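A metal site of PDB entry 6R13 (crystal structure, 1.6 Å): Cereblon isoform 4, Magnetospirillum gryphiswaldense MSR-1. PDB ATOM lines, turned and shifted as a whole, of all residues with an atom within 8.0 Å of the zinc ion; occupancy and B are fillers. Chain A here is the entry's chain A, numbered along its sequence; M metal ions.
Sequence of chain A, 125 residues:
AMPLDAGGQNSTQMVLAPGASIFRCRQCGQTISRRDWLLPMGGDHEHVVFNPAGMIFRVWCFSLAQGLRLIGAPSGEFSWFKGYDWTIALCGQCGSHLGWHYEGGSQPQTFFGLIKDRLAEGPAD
SG of Cys 94 lies close to N of Ser 96.
The side-chain sulfur (SG) of Cys 25 lies close to the backbone NH (N) of Gln 27 (3.4 Å).
The backbone NH (N) of Cys 25 is in hydrogen-bond range of the backbone carbonyl oxygen (O) of Gln 30 (2.9 Å).
The backbone NH of Gln 30 lies close to the side-chain sulfur of Cys 28 (3.6 Å).
SG of Cys 28 sits close to NE2 of Gln 93, at 3.2 Å.
The backbone NH of Cys 91 sits at hydrogen-bond distance from the backbone carbonyl oxygen of Ser 96 (2.7 Å).
The side-chain sulfur (SG) of Cys 91 sits close to the backbone NH (N) of Gln 93, at 3.5 Å.
The side-chain sulfur (SG) of Cys 94 binds the zinc ion.
The side-chain sulfur (SG) of Cys 25 binds the zinc ion.
The side-chain sulfur (SG) of Cys 28 is bound to the zinc ion.
SG of Cys 91 binds the zinc ion, at 2.3 Å.
The zinc ion has four donor atoms within binding distance.
Of the 21 residues printed, 4 come within 4 Å of the zinc ion.
The nearest printed residue that does not touch the zinc ion is Ser 96 (4.4 Å).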
ATOM      1  N   ARG A  24      23.324  -6.490  13.337  1.00  0.00           N
ATOM      2  CA  ARG A  24      22.900  -5.853  14.560  1.00  0.00           C
ATOM      3  C   ARG A  24      23.507  -6.599  15.740  1.00  0.00           C
ATOM      4  O   ARG A  24      23.864  -7.734  15.600  1.00  0.00           O
ATOM      5  CB  ARG A  24      21.381  -5.888  14.696  1.00  0.00           C
ATOM      6  CG  ARG A  24      20.651  -5.113  13.626  1.00  0.00           C
ATOM      7  CD  ARG A  24      19.143  -5.020  13.814  1.00  0.00           C
ATOM      8  NE  ARG A  24      18.587  -4.048  12.860  1.00  0.00           N
ATOM      9  CZ  ARG A  24      18.643  -2.719  12.998  1.00  0.00           C
ATOM     10  NH1 ARG A  24      19.077  -2.146  14.108  1.00  0.00           N
ATOM     11  NH2 ARG A  24      18.180  -1.951  12.021  1.00  0.00           N
ATOM     12  N   CYS A  25      23.623  -5.953  16.892  1.00  0.00           N
ATOM     13  CA  CYS A  25      24.031  -6.628  18.106  1.00  0.00           C
ATOM     14  C   CYS A  25      22.992  -7.735  18.418  1.00  0.00           C
ATOM     15  O   CYS A  25      21.801  -7.465  18.447  1.00  0.00           O
ATOM     16  CB  CYS A  25      24.090  -5.661  19.266  1.00  0.00           C
ATOM     17  SG  CYS A  25      24.412  -6.438  20.873  1.00  0.00           S
ATOM     18  N   ARG A  26      23.477  -8.956  18.628  1.00  0.00           N
ATOM     19  CA  ARG A  26      22.590 -10.075  18.900  1.00  0.00           C
ATOM     20  C   ARG A  26      21.813  -9.917  20.201  1.00  0.00           C
ATOM     21  O   ARG A  26      20.744 -10.509  20.335  1.00  0.00           O
ATOM     22  CB  ARG A  26      23.432 -11.343  18.940  1.00  0.00           C
ATOM     23  CG  ARG A  26      22.721 -12.615  19.307  1.00  0.00           C
ATOM     24  CD  ARG A  26      23.696 -13.733  19.343  1.00  0.00           C
ATOM     25  NE  ARG A  26      22.997 -14.882  19.889  1.00  0.00           N
ATOM     26  CZ  ARG A  26      23.549 -16.103  19.995  1.00  0.00           C
ATOM     27  NH1 ARG A  26      24.778 -16.355  19.548  1.00  0.00           N
ATOM     28  NH2 ARG A  26      22.839 -17.054  20.574  1.00  0.00           N
ATOM     29  N   GLN A  27      22.374  -9.181  21.157  1.00  0.00           N
ATOM     30  CA  GLN A  27      21.717  -9.017  22.475  1.00  0.00           C
ATOM     31  C   GLN A  27      20.653  -7.944  22.535  1.00  0.00           C
ATOM     32  O   GLN A  27      19.677  -8.078  23.272  1.00  0.00           O
ATOM     33  CB  GLN A  27      22.768  -8.784  23.556  1.00  0.00           C
ATOM     34  CG  GLN A  27      23.785  -9.905  23.628  1.00  0.00           C
ATOM     35  CD  GLN A  27      23.172 -11.293  23.859  1.00  0.00           C
ATOM     36  OE1 GLN A  27      22.208 -11.440  24.599  1.00  0.00           O
ATOM     37  NE2 GLN A  27      23.740 -12.306  23.226  1.00  0.00           N
ATOM     38  N   CYS A  28      20.785  -6.884  21.744  1.00  0.00           N
ATOM     39  CA  CYS A  28      19.868  -5.731  21.876  1.00  0.00           C
ATOM     40  C   CYS A  28      19.369  -5.131  20.577  1.00  0.00           C
ATOM     41  O   CYS A  28      18.470  -4.274  20.586  1.00  0.00           O
ATOM     42  CB  CYS A  28      20.547  -4.677  22.755  1.00  0.00           C
ATOM     43  SG  CYS A  28      21.791  -3.754  21.841  1.00  0.00           S
ATOM     44  N   GLY A  29      19.942  -5.510  19.426  1.00  0.00           N
ATOM     45  CA  GLY A  29      19.485  -5.011  18.160  1.00  0.00           C
ATOM     46  C   GLY A  29      20.108  -3.728  17.639  1.00  0.00           C
ATOM     47  O   GLY A  29      19.762  -3.232  16.556  1.00  0.00           O
ATOM     48  N   GLN A  30      21.031  -3.160  18.385  1.00  0.00           N
ATOM     49  CA  GLN A  30      21.751  -1.966  17.922  1.00  0.00           C
ATOM     50  C   GLN A  30      22.348  -2.207  16.552  1.00  0.00           C
ATOM     51  O   GLN A  30      22.955  -3.216  16.319  1.00  0.00           O
ATOM     52  CB  GLN A  30      22.857  -1.612  18.921  1.00  0.00           C
ATOM     53  CG  GLN A  30      23.787  -0.467  18.479  1.00  0.00           C
ATOM     54  CD  GLN A  30      23.074   0.865  18.311  1.00  0.00           C
ATOM     55  OE1 GLN A  30      22.266   1.262  19.105  1.00  0.00           O
ATOM     56  NE2 GLN A  30      23.371   1.587  17.190  1.00  0.00           N
ATOM     57  N   THR A  31      22.173  -1.259  15.637  1.00  0.00           N
ATOM     58  CA  THR A  31      22.778  -1.386  14.304  1.00  0.00           C
ATOM     59  C   THR A  31      24.278  -1.281  14.403  1.00  0.00           C
ATOM     60  O   THR A  31      24.768  -0.333  15.053  1.00  0.00           O
ATOM     61  CB  THR A  31      22.302  -0.242  13.373  1.00  0.00           C
ATOM     62  OG1 THR A  31      20.902   0.034  13.558  1.00  0.00           O
ATOM     63  CG2 THR A  31      22.581  -0.617  11.986  1.00  0.00           C
ATOM     64  N   ILE A  32      25.030  -2.210  13.794  1.00  0.00           N
ATOM     65  CA  ILE A  32      26.498  -2.237  13.968  1.00  0.00           C
ATOM     66  C   ILE A  32      27.231  -2.095  12.640  1.00  0.00           C
ATOM     67  O   ILE A  32      28.156  -1.284  12.519  1.00  0.00           O
ATOM     68  CB  ILE A  32      26.997  -3.507  14.708  1.00  0.00           C
ATOM     69  CG1 ILE A  32      26.342  -3.634  16.083  1.00  0.00           C
ATOM     70  CG2 ILE A  32      28.512  -3.486  14.853  1.00  0.00           C
ATOM     71  CD1 ILE A  32      26.646  -2.535  17.096  1.00  0.00           C
ATOM     72  N   GLY A  67      27.684   2.342  16.156  1.00  0.00           N
ATOM     73  CA  GLY A  67      26.927   1.898  17.332  1.00  0.00           C
ATOM     74  C   GLY A  67      27.772   1.192  18.381  1.00  0.00           C
ATOM     75  O   GLY A  67      27.195   0.575  19.289  1.00  0.00           O
ATOM     76  N   LEU A  68      29.094   1.263  18.258  1.00  0.00           N
ATOM     77  CA  LEU A  68      30.018   0.658  19.225  1.00  0.00           C
ATOM     78  C   LEU A  68      30.526   1.716  20.175  1.00  0.00           C
ATOM     79  O   LEU A  68      30.311   2.894  19.960  1.00  0.00           O
ATOM     80  CB  LEU A  68      31.217   0.005  18.517  1.00  0.00           C
ATOM     81  CG  LEU A  68      30.851  -1.108  17.536  1.00  0.00           C
ATOM     82  CD1 LEU A  68      31.966  -1.330  16.519  1.00  0.00           C
ATOM     83  CD2 LEU A  68      30.469  -2.387  18.291  1.00  0.00           C
ATOM     84  N   LEU A  90      32.807  -2.498  22.358  1.00  0.00           N
ATOM     85  CA  LEU A  90      31.546  -2.961  22.978  1.00  0.00           C
ATOM     86  C   LEU A  90      30.347  -2.421  22.196  1.00  0.00           C
ATOM     87  O   LEU A  90      30.422  -1.368  21.550  1.00  0.00           O
ATOM     88  CB  LEU A  90      31.455  -2.437  24.386  1.00  0.00           C
ATOM     89  CG  LEU A  90      32.574  -2.779  25.350  1.00  0.00           C
ATOM     90  CD1 LEU A  90      32.226  -2.212  26.722  1.00  0.00           C
ATOM     91  CD2 LEU A  90      32.835  -4.295  25.374  1.00  0.00           C
ATOM     92  N   CYS A  91      29.249  -3.137  22.265  1.00  0.00           N
ATOM     93  CA  CYS A  91      27.990  -2.532  21.807  1.00  0.00           C
ATOM     94  C   CYS A  91      27.756  -1.271  22.600  1.00  0.00           C
ATOM     95  O   CYS A  91      27.777  -1.282  23.840  1.00  0.00           O
ATOM     96  CB  CYS A  91      26.822  -3.504  22.015  1.00  0.00           C
ATOM     97  SG  CYS A  91      25.224  -2.801  21.594  1.00  0.00           S
ATOM     98  N   GLY A  92      27.515  -0.144  21.893  1.00  0.00           N
ATOM     99  CA  GLY A  92      27.301   1.120  22.559  1.00  0.00           C
ATOM    100  C   GLY A  92      26.012   1.223  23.338  1.00  0.00           C
ATOM    101  O   GLY A  92      25.871   2.111  24.193  1.00  0.00           O
ATOM    102  N   GLN A  93      25.071   0.325  23.049  1.00  0.00           N
ATOM    103  CA  GLN A  93      23.785   0.337  23.685  1.00  0.00           C
ATOM    104  C   GLN A  93      23.804  -0.550  24.931  1.00  0.00           C
ATOM    105  O   GLN A  93      23.493  -0.072  26.022  1.00  0.00           O
ATOM    106  CB  GLN A  93      22.729  -0.083  22.685  1.00  0.00           C
ATOM    107  CG  GLN A  93      21.313  -0.022  23.184  1.00  0.00           C
ATOM    108  CD  GLN A  93      20.315   0.013  22.047  1.00  0.00           C
ATOM    109  OE1 GLN A  93      19.826   1.084  21.764  1.00  0.00           O
ATOM    110  NE2 GLN A  93      20.050  -1.118  21.381  1.00  0.00           N
ATOM    111  N   CYS A  94      24.198  -1.810  24.754  1.00  0.00           N
ATOM    112  CA  CYS A  94      24.068  -2.812  25.844  1.00  0.00           C
ATOM    113  C   CYS A  94      25.381  -3.254  26.503  1.00  0.00           C
ATOM    114  O   CYS A  94      25.318  -3.922  27.537  1.00  0.00           O
ATOM    115  CB  CYS A  94      23.308  -4.032  25.365  1.00  0.00           C
ATOM    116  SG  CYS A  94      24.269  -5.237  24.398  1.00  0.00           S
ATOM    117  N   GLY A  95      26.532  -2.881  25.926  1.00  0.00           N
ATOM    118  CA  GLY A  95      27.806  -3.242  26.516  1.00  0.00           C
ATOM    119  C   GLY A  95      28.348  -4.614  26.115  1.00  0.00           C
ATOM    120  O   GLY A  95      29.451  -4.964  26.546  1.00  0.00           O
ATOM    121  N   SER A  96      27.626  -5.367  25.300  1.00  0.00           N
ATOM    122  CA  SER A  96      28.085  -6.690  24.814  1.00  0.00           C
ATOM    123  C   SER A  96      29.446  -6.537  24.120  1.00  0.00           C
ATOM    124  O   SER A  96      29.651  -5.604  23.341  1.00  0.00           O
ATOM    125  CB  SER A  96      27.100  -7.287  23.846  1.00  0.00           C
ATOM    126  OG  SER A  96      27.565  -8.552  23.320  1.00  0.00           O
ATOM    127  N   HIS A  97      30.396  -7.423  24.416  1.00  0.00           N
ATOM    128  CA  HIS A  97      31.698  -7.347  23.700  1.00  0.00           C
ATOM    129  C   HIS A  97      31.556  -7.888  22.298  1.00  0.00           C
ATOM    130  O   HIS A  97      31.390  -9.087  22.100  1.00  0.00           O
ATOM    131  CB  HIS A  97      32.766  -8.107  24.470  1.00  0.00           C
ATOM    132  CG  HIS A  97      34.067  -8.123  23.757  1.00  0.00           C
ATOM    133  ND1 HIS A  97      34.954  -9.173  23.880  1.00  0.00           N
ATOM    134  CD2 HIS A  97      34.639  -7.244  22.909  1.00  0.00           C
ATOM    135  CE1 HIS A  97      36.035  -8.915  23.165  1.00  0.00           C
ATOM    136  NE2 HIS A  97      35.855  -7.775  22.530  1.00  0.00           N
ATOM    137  N   LEU A  98      31.605  -7.015  21.304  1.00  0.00           N
ATOM    138  CA  LEU A  98      31.360  -7.426  19.918  1.00  0.00           C
ATOM    139  C   LEU A  98      32.586  -7.664  19.085  1.00  0.00           C
ATOM    140  O   LEU A  98      32.511  -8.319  18.035  1.00  0.00           O
ATOM    141  CB  LEU A  98      30.469  -6.426  19.206  1.00  0.00           C
ATOM    142  CG  LEU A  98      29.066  -6.278  19.831  1.00  0.00           C
ATOM    143  CD1 LEU A  98      28.230  -5.387  18.954  1.00  0.00           C
ATOM    144  CD2 LEU A  98      28.393  -7.603  20.000  1.00  0.00           C
ATOM    145  N   ARG A 118      28.225 -13.061  17.670  1.00  0.00           N
ATOM    146  CA  ARG A 118      27.682 -12.024  18.542  1.00  0.00           C
ATOM    147  C   ARG A 118      26.846 -10.983  17.812  1.00  0.00           C
ATOM    148  O   ARG A 118      26.357 -10.026  18.416  1.00  0.00           O
ATOM    149  CB  ARG A 118      28.797 -11.378  19.353  1.00  0.00           C
ATOM    150  CG  ARG A 118      29.447 -12.453  20.215  1.00  0.00           C
ATOM    151  CD  ARG A 118      30.402 -11.917  21.231  1.00  0.00           C
ATOM    152  NE  ARG A 118      31.151 -12.988  21.881  1.00  0.00           N
ATOM    153  CZ  ARG A 118      32.048 -12.800  22.866  1.00  0.00           C
ATOM    154  NH1 ARG A 118      32.313 -11.576  23.335  1.00  0.00           N
ATOM    155  NH2 ARG A 118      32.679 -13.834  23.412  1.00  0.00           N
HETATM  156 ZN    ZN M   1      23.920  -4.641  22.218  1.00  0.00          ZN
